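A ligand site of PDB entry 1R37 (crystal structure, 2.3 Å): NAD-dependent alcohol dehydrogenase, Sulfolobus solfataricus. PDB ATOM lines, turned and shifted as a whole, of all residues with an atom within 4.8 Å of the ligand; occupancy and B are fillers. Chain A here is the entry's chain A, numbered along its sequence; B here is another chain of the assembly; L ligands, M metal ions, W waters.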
ATOM      1  N   CYS A  38      -7.058   7.385   2.076  1.00  0.00           N
ATOM      2  CA  CYS A  38      -8.061   7.163   3.097  1.00  0.00           C
ATOM      3  C   CYS A  38      -7.985   8.216   4.206  1.00  0.00           C
ATOM      4  O   CYS A  38      -6.910   8.702   4.538  1.00  0.00           O
ATOM      5  CB  CYS A  38      -7.838   5.779   3.697  1.00  0.00           C
ATOM      6  SG  CYS A  38      -9.078   5.279   4.920  1.00  0.00           S
ATOM      7  N   HIS A  39      -9.129   8.548   4.813  1.00  0.00           N
ATOM      8  CA  HIS A  39      -9.133   9.542   5.873  1.00  0.00           C
ATOM      9  C   HIS A  39      -8.309   9.038   7.066  1.00  0.00           C
ATOM     10  O   HIS A  39      -7.948   9.810   7.957  1.00  0.00           O
ATOM     11  CB  HIS A  39     -10.572   9.866   6.302  1.00  0.00           C
ATOM     12  CG  HIS A  39     -10.705  11.122   7.114  1.00  0.00           C
ATOM     13  ND1 HIS A  39     -11.497  12.183   6.721  1.00  0.00           N
ATOM     14  CD2 HIS A  39     -10.170  11.476   8.309  1.00  0.00           C
ATOM     15  CE1 HIS A  39     -11.438  13.132   7.637  1.00  0.00           C
ATOM     16  NE2 HIS A  39     -10.644  12.729   8.610  1.00  0.00           N
ATOM     17  N   SER A  40      -7.993   7.737   7.086  1.00  0.00           N
ATOM     18  CA  SER A  40      -7.137   7.183   8.139  1.00  0.00           C
ATOM     19  C   SER A  40      -5.736   7.768   8.064  1.00  0.00           C
ATOM     20  O   SER A  40      -5.030   7.858   9.076  1.00  0.00           O
ATOM     21  CB  SER A  40      -7.039   5.657   8.024  1.00  0.00           C
ATOM     22  OG  SER A  40      -8.209   5.014   8.480  1.00  0.00           O
ATOM     23  N   HIS A  43      -5.291  10.742  10.215  1.00  0.00           N
ATOM     24  CA  HIS A  43      -5.034  10.399  11.615  1.00  0.00           C
ATOM     25  C   HIS A  43      -3.594   9.949  11.778  1.00  0.00           C
ATOM     26  O   HIS A  43      -2.938  10.268  12.774  1.00  0.00           O
ATOM     27  CB  HIS A  43      -5.981   9.282  12.066  1.00  0.00           C
ATOM     28  CG  HIS A  43      -7.436   9.576  11.849  1.00  0.00           C
ATOM     29  ND1 HIS A  43      -8.029  10.748  12.267  1.00  0.00           N
ATOM     30  CD2 HIS A  43      -8.418   8.842  11.263  1.00  0.00           C
ATOM     31  CE1 HIS A  43      -9.317  10.715  11.948  1.00  0.00           C
ATOM     32  NE2 HIS A  43      -9.578   9.580  11.340  1.00  0.00           N
ATOM     33  N   PHE A  49      -5.283   7.923  16.583  1.00  0.00           N
ATOM     34  CA  PHE A  49      -6.693   7.655  16.337  1.00  0.00           C
ATOM     35  C   PHE A  49      -7.313   7.866  17.713  1.00  0.00           C
ATOM     36  O   PHE A  49      -7.165   7.023  18.592  1.00  0.00           O
ATOM     37  CB  PHE A  49      -6.893   6.206  15.893  1.00  0.00           C
ATOM     38  CG  PHE A  49      -6.292   5.894  14.550  1.00  0.00           C
ATOM     39  CD1 PHE A  49      -6.993   6.161  13.377  1.00  0.00           C
ATOM     40  CD2 PHE A  49      -5.031   5.338  14.454  1.00  0.00           C
ATOM     41  CE1 PHE A  49      -6.442   5.867  12.118  1.00  0.00           C
ATOM     42  CE2 PHE A  49      -4.468   5.037  13.201  1.00  0.00           C
ATOM     43  CZ  PHE A  49      -5.177   5.313  12.036  1.00  0.00           C
ATOM     44  N   CYS A 154      -9.680  -1.234   1.201  1.00  0.00           N
ATOM     45  CA  CYS A 154      -9.928  -0.627   2.502  1.00  0.00           C
ATOM     46  C   CYS A 154     -11.378  -0.185   2.620  1.00  0.00           C
ATOM     47  O   CYS A 154     -12.152  -0.787   3.354  1.00  0.00           O
ATOM     48  CB  CYS A 154      -9.024   0.566   2.779  1.00  0.00           C
ATOM     49  SG  CYS A 154      -9.359   1.179   4.460  1.00  0.00           S
ATOM     50  N   THR A 158     -13.865  -2.841   4.305  1.00  0.00           N
ATOM     51  CA  THR A 158     -14.322  -2.362   5.598  1.00  0.00           C
ATOM     52  C   THR A 158     -15.835  -2.217   5.635  1.00  0.00           C
ATOM     53  O   THR A 158     -16.491  -2.669   6.583  1.00  0.00           O
ATOM     54  CB  THR A 158     -13.735  -0.973   5.954  1.00  0.00           C
ATOM     55  OG1 THR A 158     -12.314  -1.058   6.102  1.00  0.00           O
ATOM     56  CG2 THR A 158     -14.343  -0.461   7.252  1.00  0.00           C
ATOM     57  N   VAL A 177     -23.956   7.200   8.354  1.00  0.00           N
ATOM     58  CA  VAL A 177     -23.550   8.515   8.834  1.00  0.00           C
ATOM     59  C   VAL A 177     -22.232   8.913   8.177  1.00  0.00           C
ATOM     60  O   VAL A 177     -21.220   8.257   8.385  1.00  0.00           O
ATOM     61  CB  VAL A 177     -23.381   8.517  10.392  1.00  0.00           C
ATOM     62  CG1 VAL A 177     -23.019   9.914  10.876  1.00  0.00           C
ATOM     63  CG2 VAL A 177     -24.681   8.063  11.056  1.00  0.00           C
ATOM     64  N   GLY A 178     -22.262   9.998   7.404  1.00  0.00           N
ATOM     65  CA  GLY A 178     -21.068  10.431   6.699  1.00  0.00           C
ATOM     66  C   GLY A 178     -21.094   9.715   5.369  1.00  0.00           C
ATOM     67  O   GLY A 178     -20.064   9.311   4.822  1.00  0.00           O
ATOM     68  N   GLY A 180     -21.512  10.631   2.363  1.00  0.00           N
ATOM     69  CA  GLY A 180     -20.991  11.232   1.138  1.00  0.00           C
ATOM     70  C   GLY A 180     -19.495  11.073   0.959  1.00  0.00           C
ATOM     71  O   GLY A 180     -18.950  11.508  -0.053  1.00  0.00           O
ATOM     72  N   GLY A 181     -18.831  10.448   1.929  1.00  0.00           N
ATOM     73  CA  GLY A 181     -17.385  10.294   1.875  1.00  0.00           C
ATOM     74  C   GLY A 181     -16.885   9.016   1.205  1.00  0.00           C
ATOM     75  O   GLY A 181     -17.644   8.321   0.513  1.00  0.00           O
ATOM     76  N   GLY A 182     -15.611   8.701   1.409  1.00  0.00           N
ATOM     77  CA  GLY A 182     -15.025   7.514   0.810  1.00  0.00           C
ATOM     78  C   GLY A 182     -15.722   6.221   1.196  1.00  0.00           C
ATOM     79  O   GLY A 182     -16.129   5.447   0.326  1.00  0.00           O
ATOM     80  N   LEU A 183     -15.844   5.982   2.501  1.00  0.00           N
ATOM     81  CA  LEU A 183     -16.512   4.770   2.976  1.00  0.00           C
ATOM     82  C   LEU A 183     -18.021   4.908   2.871  1.00  0.00           C
ATOM     83  O   LEU A 183     -18.723   3.934   2.554  1.00  0.00           O
ATOM     84  CB  LEU A 183     -16.131   4.481   4.436  1.00  0.00           C
ATOM     85  CG  LEU A 183     -14.820   3.715   4.629  1.00  0.00           C
ATOM     86  CD1 LEU A 183     -13.654   4.603   4.207  1.00  0.00           C
ATOM     87  CD2 LEU A 183     -14.669   3.277   6.084  1.00  0.00           C
ATOM     88  N   GLY A 184     -18.519   6.110   3.130  1.00  0.00           N
ATOM     89  CA  GLY A 184     -19.947   6.357   3.071  1.00  0.00           C
ATOM     90  C   GLY A 184     -20.572   5.970   1.737  1.00  0.00           C
ATOM     91  O   GLY A 184     -21.583   5.276   1.704  1.00  0.00           O
ATOM     92  N   VAL A 202     -26.831  10.186   5.683  1.00  0.00           N
ATOM     93  CA  VAL A 202     -26.797  11.518   6.278  1.00  0.00           C
ATOM     94  C   VAL A 202     -25.395  12.112   6.208  1.00  0.00           C
ATOM     95  O   VAL A 202     -24.403  11.416   6.468  1.00  0.00           O
ATOM     96  CB  VAL A 202     -27.258  11.505   7.773  1.00  0.00           C
ATOM     97  CG1 VAL A 202     -26.326  10.623   8.609  1.00  0.00           C
ATOM     98  CG2 VAL A 202     -27.281  12.915   8.324  1.00  0.00           C
ATOM     99  N   ASP A 203     -25.299  13.375   5.829  1.00  0.00           N
ATOM    100  CA  ASP A 203     -24.024  14.073   5.796  1.00  0.00           C
ATOM    101  C   ASP A 203     -24.310  15.544   6.122  1.00  0.00           C
ATOM    102  O   ASP A 203     -25.443  15.898   6.447  1.00  0.00           O
ATOM    103  CB  ASP A 203     -23.357  13.920   4.426  1.00  0.00           C
ATOM    104  CG  ASP A 203     -21.844  13.915   4.510  1.00  0.00           C
ATOM    105  OD1 ASP A 203     -21.285  14.936   4.977  1.00  0.00           O
ATOM    106  OD2 ASP A 203     -21.206  12.896   4.139  1.00  0.00           O
ATOM    107  N   VAL A 204     -23.299  16.407   6.063  1.00  0.00           N
ATOM    108  CA  VAL A 204     -23.504  17.801   6.442  1.00  0.00           C
ATOM    109  C   VAL A 204     -22.994  18.810   5.416  1.00  0.00           C
ATOM    110  O   VAL A 204     -22.816  19.996   5.731  1.00  0.00           O
ATOM    111  CB  VAL A 204     -22.848  18.078   7.804  1.00  0.00           C
ATOM    112  CG1 VAL A 204     -23.487  17.192   8.856  1.00  0.00           C
ATOM    113  CG2 VAL A 204     -21.354  17.817   7.728  1.00  0.00           C
ATOM    114  N   ARG A 205     -22.754  18.330   4.205  1.00  0.00           N
ATOM    115  CA  ARG A 205     -22.306  19.182   3.108  1.00  0.00           C
ATOM    116  C   ARG A 205     -23.173  18.840   1.906  1.00  0.00           C
ATOM    117  O   ARG A 205     -23.463  17.665   1.635  1.00  0.00           O
ATOM    118  CB  ARG A 205     -20.827  18.906   2.778  1.00  0.00           C
ATOM    119  CG  ARG A 205     -19.836  19.407   3.817  1.00  0.00           C
ATOM    120  CD  ARG A 205     -18.407  19.042   3.436  1.00  0.00           C
ATOM    121  NE  ARG A 205     -18.202  17.588   3.434  1.00  0.00           N
ATOM    122  CZ  ARG A 205     -17.641  16.920   2.434  1.00  0.00           C
ATOM    123  NH1 ARG A 205     -17.227  17.557   1.343  1.00  0.00           N
ATOM    124  NH2 ARG A 205     -17.495  15.601   2.526  1.00  0.00           N
ATOM    125  N   ALA A 208     -21.795  16.330  -0.457  1.00  0.00           N
ATOM    126  CA  ALA A 208     -21.689  15.015   0.153  1.00  0.00           C
ATOM    127  C   ALA A 208     -23.063  14.335   0.120  1.00  0.00           C
ATOM    128  O   ALA A 208     -23.171  13.153  -0.207  1.00  0.00           O
ATOM    129  CB  ALA A 208     -21.192  15.137   1.589  1.00  0.00           C
ATOM    130  N   LEU A 247     -19.512   6.333  10.100  1.00  0.00           N
ATOM    131  CA  LEU A 247     -18.174   6.458   9.558  1.00  0.00           C
ATOM    132  C   LEU A 247     -17.461   7.711  10.116  1.00  0.00           C
ATOM    133  O   LEU A 247     -16.570   8.252   9.488  1.00  0.00           O
ATOM    134  CB  LEU A 247     -18.267   6.512   8.035  1.00  0.00           C
ATOM    135  CG  LEU A 247     -19.029   5.296   7.476  1.00  0.00           C
ATOM    136  CD1 LEU A 247     -19.551   5.613   6.102  1.00  0.00           C
ATOM    137  CD2 LEU A 247     -18.128   4.076   7.454  1.00  0.00           C
ATOM    138  N   ASN A 248     -17.886   8.140  11.305  1.00  0.00           N
ATOM    139  CA  ASN A 248     -17.281   9.285  11.996  1.00  0.00           C
ATOM    140  C   ASN A 248     -16.913   8.918  13.430  1.00  0.00           C
ATOM    141  O   ASN A 248     -15.743   8.890  13.793  1.00  0.00           O
ATOM    142  CB  ASN A 248     -18.256  10.458  12.026  1.00  0.00           C
ATOM    143  CG  ASN A 248     -18.252  11.280  10.743  1.00  0.00           C
ATOM    144  OD1 ASN A 248     -17.906  10.774   9.665  1.00  0.00           O
ATOM    145  ND2 ASN A 248     -18.629  12.537  10.854  1.00  0.00           N
ATOM    146  N   LYS A 252     -20.081  14.594  17.821  1.00  0.00           N
ATOM    147  CA  LYS A 252     -21.228  15.090  17.061  1.00  0.00           C
ATOM    148  C   LYS A 252     -22.146  13.974  16.592  1.00  0.00           C
ATOM    149  O   LYS A 252     -23.365  14.129  16.599  1.00  0.00           O
ATOM    150  CB  LYS A 252     -20.761  15.903  15.847  1.00  0.00           C
ATOM    151  CG  LYS A 252     -19.945  17.136  16.171  1.00  0.00           C
ATOM    152  CD  LYS A 252     -19.679  17.936  14.903  1.00  0.00           C
ATOM    153  CE  LYS A 252     -18.941  19.235  15.190  1.00  0.00           C
ATOM    154  NZ  LYS A 252     -18.887  20.105  13.967  1.00  0.00           N
ATOM    155  N   THR A 253     -21.576  12.849  16.149  1.00  0.00           N
ATOM    156  CA  THR A 253     -22.434  11.765  15.703  1.00  0.00           C
ATOM    157  C   THR A 253     -22.882  10.867  16.854  1.00  0.00           C
ATOM    158  O   THR A 253     -24.065  10.525  16.941  1.00  0.00           O
ATOM    159  CB  THR A 253     -21.774  10.898  14.580  1.00  0.00           C
ATOM    160  OG1 THR A 253     -20.605  10.225  15.077  1.00  0.00           O
ATOM    161  CG2 THR A 253     -21.395  11.779  13.406  1.00  0.00           C
ATOM    162  N   VAL A 270     -17.380   2.381  12.814  1.00  0.00           N
ATOM    163  CA  VAL A 270     -16.273   2.307  11.875  1.00  0.00           C
ATOM    164  C   VAL A 270     -15.376   3.546  11.914  1.00  0.00           C
ATOM    165  O   VAL A 270     -14.153   3.427  11.907  1.00  0.00           O
ATOM    166  CB  VAL A 270     -16.822   2.097  10.425  1.00  0.00           C
ATOM    167  CG1 VAL A 270     -15.704   2.166   9.409  1.00  0.00           C
ATOM    168  CG2 VAL A 270     -17.536   0.742  10.328  1.00  0.00           C
ATOM    169  N   GLY A 271     -15.986   4.726  11.947  1.00  0.00           N
ATOM    170  CA  GLY A 271     -15.221   5.968  11.954  1.00  0.00           C
ATOM    171  C   GLY A 271     -14.251   6.094  13.096  1.00  0.00           C
ATOM    172  O   GLY A 271     -14.467   5.528  14.170  1.00  0.00           O
ATOM    173  N   LEU A 272     -13.163   6.839  12.889  1.00  0.00           N
ATOM    174  CA  LEU A 272     -12.139   6.990  13.914  1.00  0.00           C
ATOM    175  C   LEU A 272     -11.823   8.431  14.289  1.00  0.00           C
ATOM    176  O   LEU A 272     -10.675   8.765  14.624  1.00  0.00           O
ATOM    177  CB  LEU A 272     -10.873   6.258  13.448  1.00  0.00           C
ATOM    178  CG  LEU A 272     -11.016   4.735  13.324  1.00  0.00           C
ATOM    179  CD1 LEU A 272      -9.859   4.180  12.510  1.00  0.00           C
ATOM    180  CD2 LEU A 272     -11.059   4.088  14.725  1.00  0.00           C
ATOM    181  N   PHE A 273     -12.836   9.302  14.255  1.00  0.00           N
ATOM    182  CA  PHE A 273     -12.628  10.714  14.584  1.00  0.00           C
ATOM    183  C   PHE A 273     -12.154  10.910  16.028  1.00  0.00           C
ATOM    184  O   PHE A 273     -11.599  11.961  16.355  1.00  0.00           O
ATOM    185  CB  PHE A 273     -13.906  11.513  14.309  1.00  0.00           C
ATOM    186  CG  PHE A 273     -14.164  11.785  12.848  1.00  0.00           C
ATOM    187  CD1 PHE A 273     -13.434  11.117  11.860  1.00  0.00           C
ATOM    188  CD2 PHE A 273     -15.135  12.684  12.453  1.00  0.00           C
ATOM    189  CE1 PHE A 273     -13.685  11.348  10.518  1.00  0.00           C
ATOM    190  CE2 PHE A 273     -15.395  12.930  11.110  1.00  0.00           C
ATOM    191  CZ  PHE A 273     -14.671  12.265  10.139  1.00  0.00           C
ATOM    192  N   SER A 294     -16.101  -2.424  14.079  1.00  0.00           N
ATOM    193  CA  SER A 294     -15.766  -3.172  12.873  1.00  0.00           C
ATOM    194  C   SER A 294     -14.451  -2.610  12.355  1.00  0.00           C
ATOM    195  O   SER A 294     -14.304  -1.398  12.188  1.00  0.00           O
ATOM    196  CB  SER A 294     -16.875  -3.014  11.833  1.00  0.00           C
ATOM    197  OG  SER A 294     -16.797  -4.054  10.874  1.00  0.00           O
ATOM    198  N   LEU A 295     -13.493  -3.488  12.100  1.00  0.00           N
ATOM    199  CA  LEU A 295     -12.169  -3.090  11.628  1.00  0.00           C
ATOM    200  C   LEU A 295     -11.851  -3.763  10.292  1.00  0.00           C
ATOM    201  O   LEU A 295     -11.841  -4.988  10.194  1.00  0.00           O
ATOM    202  CB  LEU A 295     -11.117  -3.477  12.668  1.00  0.00           C
ATOM    203  CG  LEU A 295      -9.667  -3.055  12.470  1.00  0.00           C
ATOM    204  CD1 LEU A 295      -9.569  -1.530  12.382  1.00  0.00           C
ATOM    205  CD2 LEU A 295      -8.823  -3.588  13.626  1.00  0.00           C
ATOM    206  N   VAL A 296     -11.580  -2.948   9.280  1.00  0.00           N
ATOM    207  CA  VAL A 296     -11.259  -3.413   7.940  1.00  0.00           C
ATOM    208  C   VAL A 296     -11.951  -4.738   7.600  1.00  0.00           C
ATOM    209  O   VAL A 296     -13.171  -4.802   7.627  1.00  0.00           O
ATOM    210  CB  VAL A 296      -9.719  -3.502   7.750  1.00  0.00           C
ATOM    211  CG1 VAL A 296      -9.131  -2.096   7.946  1.00  0.00           C
ATOM    212  CG2 VAL A 296      -9.081  -4.473   8.758  1.00  0.00           C
ATOM    213  N   LEU A 334      -9.210  15.732   2.795  1.00  0.00           N
ATOM    214  CA  LEU A 334     -10.014  14.943   3.702  1.00  0.00           C
ATOM    215  C   LEU A 334     -10.034  15.595   5.072  1.00  0.00           C
ATOM    216  O   LEU A 334     -11.082  15.674   5.718  1.00  0.00           O
ATOM    217  CB  LEU A 334      -9.461  13.515   3.793  1.00  0.00           C
ATOM    218  CG  LEU A 334      -9.568  12.713   2.495  1.00  0.00           C
ATOM    219  CD1 LEU A 334      -8.978  11.325   2.680  1.00  0.00           C
ATOM    220  CD2 LEU A 334     -11.029  12.609   2.089  1.00  0.00           C
ATOM    221  N   PHE A 337     -12.322  18.301   4.886  1.00  0.00           N
ATOM    222  CA  PHE A 337     -13.623  17.879   4.386  1.00  0.00           C
ATOM    223  C   PHE A 337     -13.988  18.566   3.075  1.00  0.00           C
ATOM    224  O   PHE A 337     -15.122  19.000   2.898  1.00  0.00           O
ATOM    225  CB  PHE A 337     -14.701  18.138   5.423  1.00  0.00           C
ATOM    226  CG  PHE A 337     -14.508  17.373   6.692  1.00  0.00           C
ATOM    227  CD1 PHE A 337     -14.145  18.028   7.860  1.00  0.00           C
ATOM    228  CD2 PHE A 337     -14.675  15.995   6.711  1.00  0.00           C
ATOM    229  CE1 PHE A 337     -13.938  17.312   9.048  1.00  0.00           C
ATOM    230  CE2 PHE A 337     -14.485  15.260   7.878  1.00  0.00           C
ATOM    231  CZ  PHE A 337     -14.109  15.931   9.054  1.00  0.00           C
ATOM    232  N   ALA A 339     -13.665  17.048   0.127  1.00  0.00           N
ATOM    233  CA  ALA A 339     -13.693  15.960  -0.831  1.00  0.00           C
ATOM    234  C   ALA A 339     -14.935  15.109  -0.627  1.00  0.00           C
ATOM    235  O   ALA A 339     -15.514  15.086   0.455  1.00  0.00           O
ATOM    236  CB  ALA A 339     -12.459  15.096  -0.665  1.00  0.00           C
ATOM    237  N   GLY A 341     -16.720  11.153  -2.127  1.00  0.00           N
ATOM    238  CA  GLY A 341     -16.321   9.908  -2.753  1.00  0.00           C
ATOM    239  C   GLY A 341     -14.892   9.572  -2.386  1.00  0.00           C
ATOM    240  O   GLY A 341     -14.475   9.794  -1.246  1.00  0.00           O
ATOM    241  N   ARG A 342     -14.112   9.067  -3.345  1.00  0.00           N
ATOM    242  CA  ARG A 342     -12.748   8.646  -3.085  1.00  0.00           C
ATOM    243  C   ARG A 342     -11.709   9.291  -4.006  1.00  0.00           C
ATOM    244  O   ARG A 342     -11.970   9.519  -5.188  1.00  0.00           O
ATOM    245  CB  ARG A 342     -12.665   7.123  -3.219  1.00  0.00           C
ATOM    246  CG  ARG A 342     -11.505   6.470  -2.484  1.00  0.00           C
ATOM    247  CD  ARG A 342     -11.487   6.929  -1.034  1.00  0.00           C
ATOM    248  NE  ARG A 342     -11.060   5.889  -0.104  1.00  0.00           N
ATOM    249  CZ  ARG A 342     -11.111   6.026   1.212  1.00  0.00           C
ATOM    250  NH1 ARG A 342     -11.563   7.161   1.748  1.00  0.00           N
ATOM    251  NH2 ARG A 342     -10.716   5.032   2.008  1.00  0.00           N
ATOM    252  N   THR B 285     -13.625   0.170  18.046  1.00  0.00           N
ATOM    253  CA  THR B 285     -13.412  -0.133  16.643  1.00  0.00           C
ATOM    254  C   THR B 285     -12.175  -1.003  16.384  1.00  0.00           C
ATOM    255  O   THR B 285     -12.274  -2.055  15.738  1.00  0.00           O
ATOM    256  CB  THR B 285     -13.290   1.167  15.839  1.00  0.00           C
ATOM    257  OG1 THR B 285     -14.500   1.929  15.992  1.00  0.00           O
ATOM    258  CG2 THR B 285     -13.075   0.878  14.359  1.00  0.00           C
HETATM  259  P1  LIG L   1     -14.041  10.984   4.253  1.00  0.00           P
HETATM  260  O1  LIG L   1     -14.008  10.538   2.838  1.00  0.00           O
HETATM  261  O2  LIG L   1     -13.328  12.241   4.653  1.00  0.00           O
HETATM  262  O3  LIG L   1     -15.571  11.050   4.646  1.00  0.00           O
HETATM  263  C1  LIG L   1     -16.055  11.498   5.960  1.00  0.00           C
HETATM  264  C2  LIG L   1     -17.432  12.062   5.728  1.00  0.00           C
HETATM  265  O4  LIG L   1     -17.925  12.505   7.053  1.00  0.00           O
HETATM  266  C3  LIG L   1     -17.501  13.360   4.827  1.00  0.00           C
HETATM  267  O5  LIG L   1     -18.344  13.117   3.651  1.00  0.00           O
HETATM  268  C4  LIG L   1     -18.025  14.456   5.734  1.00  0.00           C
HETATM  269  O6  LIG L   1     -18.758  15.498   5.178  1.00  0.00           O
HETATM  270  C5  LIG L   1     -18.775  13.608   6.786  1.00  0.00           C
HETATM  271  N1  LIG L   1     -18.988  14.340   8.030  1.00  0.00           N
HETATM  272  C6  LIG L   1     -18.203  15.231   8.766  1.00  0.00           C
HETATM  273  N2  LIG L   1     -18.806  15.674   9.867  1.00  0.00           N
HETATM  274  C7  LIG L   1     -20.015  15.095   9.918  1.00  0.00           C
HETATM  275  C8  LIG L   1     -21.137  15.173  10.876  1.00  0.00           C
HETATM  276  N3  LIG L   1     -21.111  15.939  11.957  1.00  0.00           N
HETATM  277  N4  LIG L   1     -22.242  14.400  10.548  1.00  0.00           N
HETATM  278  C9  LIG L   1     -22.342  13.613   9.469  1.00  0.00           C
HETATM  279  N5  LIG L   1     -21.311  13.497   8.529  1.00  0.00           N
HETATM  280  C10 LIG L   1     -20.163  14.256   8.788  1.00  0.00           C
HETATM  281  O7  LIG L   1     -13.460   9.844   5.168  1.00  0.00           O
HETATM  282  P2  LIG L   1     -13.370   8.229   5.006  1.00  0.00           P
HETATM  283  O8  LIG L   1     -12.175   7.872   4.247  1.00  0.00           O
HETATM  284  O9  LIG L   1     -14.717   7.805   4.490  1.00  0.00           O
HETATM  285  O10 LIG L   1     -13.091   7.814   6.548  1.00  0.00           O
HETATM  286  C11 LIG L   1     -14.092   8.055   7.605  1.00  0.00           C
HETATM  287  C12 LIG L   1     -13.586   7.527   8.898  1.00  0.00           C
HETATM  288  O11 LIG L   1     -13.444   6.056   8.776  1.00  0.00           O
HETATM  289  C13 LIG L   1     -12.144   8.024   9.322  1.00  0.00           C
HETATM  290  O12 LIG L   1     -12.106   8.378  10.720  1.00  0.00           O
HETATM  291  C14 LIG L   1     -11.238   6.810   9.043  1.00  0.00           C
HETATM  292  O13 LIG L   1     -10.034   6.796   9.767  1.00  0.00           O
HETATM  293  C15 LIG L   1     -12.211   5.619   9.373  1.00  0.00           C
HETATM  294  N6  LIG L   1     -11.892   4.315   8.736  1.00  0.00           N
HETATM  295  C16 LIG L   1     -12.068   3.139   9.538  1.00  0.00           C
HETATM  296  C17 LIG L   1     -11.822   1.914   9.070  1.00  0.00           C
HETATM  297  C18 LIG L   1     -12.025   0.687   9.942  1.00  0.00           C
HETATM  298  O14 LIG L   1     -11.460  -0.370   9.621  1.00  0.00           O
HETATM  299  N7  LIG L   1     -12.812   0.771  11.030  1.00  0.00           N
HETATM  300  C19 LIG L   1     -11.323   1.658   7.639  1.00  0.00           C
HETATM  301  C20 LIG L   1     -11.146   2.931   6.817  1.00  0.00           C
HETATM  302  C21 LIG L   1     -11.432   4.208   7.391  1.00  0.00           C
HETATM  303 ZN    ZN M   1      -8.339   3.122   5.171  1.00  0.00          ZN
HETATM  304  O   HOH W   1     -14.696  12.656   1.006  1.00  0.00           O
HETATM  305  O   HOH W   2     -24.445  14.514  12.118  1.00  0.00           O
HETATM  306  O   HOH W   3     -17.345   8.313   4.359  1.00  0.00           O
HETATM  307  O   HOH W   4     -23.864  16.649  13.240  1.00  0.00           O
HETATM  308  O   HOH W   5     -18.416  14.209  12.758  1.00  0.00           O
HETATM  309  O   HOH W   6     -13.973  14.704   3.248  1.00  0.00           O
HETATM  310  O   HOH W   7     -12.323   9.899   0.657  1.00  0.00           O
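OD1 of Asp 203 is in hydrogen-bond range of O6 of the ligand, 2.6 Å away.
An oxygen (O14) of the ligand sits at hydrogen-bond distance from the backbone NH (N) of Val 296 (2.6 Å).
An oxygen (O8) of the ligand lies within salt-bridge range of the guanidinium group (NH1) of Arg 342 (2.7 Å).
N of His 39 lies within hydrogen-bond range of O8 of the ligand, at 3.2 Å.
O2 of the ligand is in hydrogen-bond range of ND1 of His 39, at 2.8 Å.
NE of Arg 205 sits at hydrogen-bond distance from O6 of the ligand (2.8 Å).
N of Gly 182 is in hydrogen-bond range of O1 of the ligand.
The backbone NH (N) of Ser 40 lies close to an oxygen (O13) of the ligand (3.5 Å).
An oxygen (O13) of the ligand sits at hydrogen-bond distance from the side-chain hydroxyl of Ser 40 (2.9 Å).
N of Leu 272 is in hydrogen-bond range of O12 of the ligand.
NE2 of His 43 lies within hydrogen-bond range of O12 of the ligand (2.9 Å).
The backbone carbonyl oxygen (O) of Ser 294 is in hydrogen-bond range of a nitrogen (N7) of the ligand, 2.9 Å away.
N of Leu 183 is in hydrogen-bond range of O9 of the ligand, at 2.9 Å.
The side-chain amide oxygen of Asn 248 sits close to an oxygen (O4) of the ligand (3.1 Å).
The backbone carbonyl oxygen (O) of Val 270 is in hydrogen-bond range of a nitrogen (N7) of the ligand, 3.1 Å away.
The backbone NH of Gly 181 lies within hydrogen-bond range of an oxygen (O5) of the ligand (3.2 Å).
The side-chain carboxylate (OD2) of Asp 203 lies within hydrogen-bond range of the backbone NH (N) of Gly 180 (2.9 Å).
NH2 of Arg 342 lies close to SG of Cys 38 (3.4 Å).
The backbone carbonyl oxygen (O) of Phe 337 is in hydrogen-bond range of the guanidinium group (NH1) of Arg 205 (3.0 Å).
The backbone carbonyl oxygen (O) of Ala 339 lies within hydrogen-bond range of the guanidinium group (NH2) of Arg 205, 2.9 Å away.
O of Gly 341 is in hydrogen-bond range of N of Gly 182, at 3.1 Å.
SG of Cys 38 sits close to N of Ser 40 (3.5 Å).
The backbone NH (N) of Leu 247 is in hydrogen-bond range of the backbone carbonyl oxygen (O) of Val 177.
O of Cys 154 lies within hydrogen-bond range of OG1 of Thr 158, 2.8 Å away.
Residues that only touch the ligand: Leu 247 (3.1 Å), Phe 273 (3.3 Å), Thr 158 (3.3 Å), Thr 285 of chain B (3.3 Å), Cys 154 (3.4 Å), Leu 295 (3.5 Å), Leu 334 (3.5 Å), Val 204 (3.5 Å), Gly 180 (3.6 Å), Cys 38 (3.6 Å), Gly 178 (3.6 Å), Gly 271 (3.6 Å), Phe 337 (3.8 Å), Lys 252 (3.8 Å) and Thr 253 (3.97 Å).
Hydrophobic or aromatic side chains within 4 Å of the ligand: His 39, His 43, Leu 183, Val 204, Val 270, Leu 272, Phe 273, Leu 295, Val 296, Leu 334 and Phe 337.
Of the 36 residues printed, 29 come within 4 Å of the ligand.
The nearest printed residue that does not touch the ligand is Val 177 (4.02 Å).
Water W7 lies within hydrogen-bond range of an oxygen (O1) of the ligand (2.8 Å), the backbone carbonyl oxygen of Gly 341 (2.9 Å) and the guanidinium group of Arg 342 (3.0 Å).
Water W1 lies within hydrogen-bond range of O of Ala 339 (2.6 Å) and O1 of the ligand (2.9 Å).
Water W6 bridges O2 of the ligand (2.9 Å) and O of Ala 339 (3.2 Å).
Water W5 lies within hydrogen-bond range of ND2 of Asn 248 (2.5 Å) and N2 of the ligand (3.3 Å).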
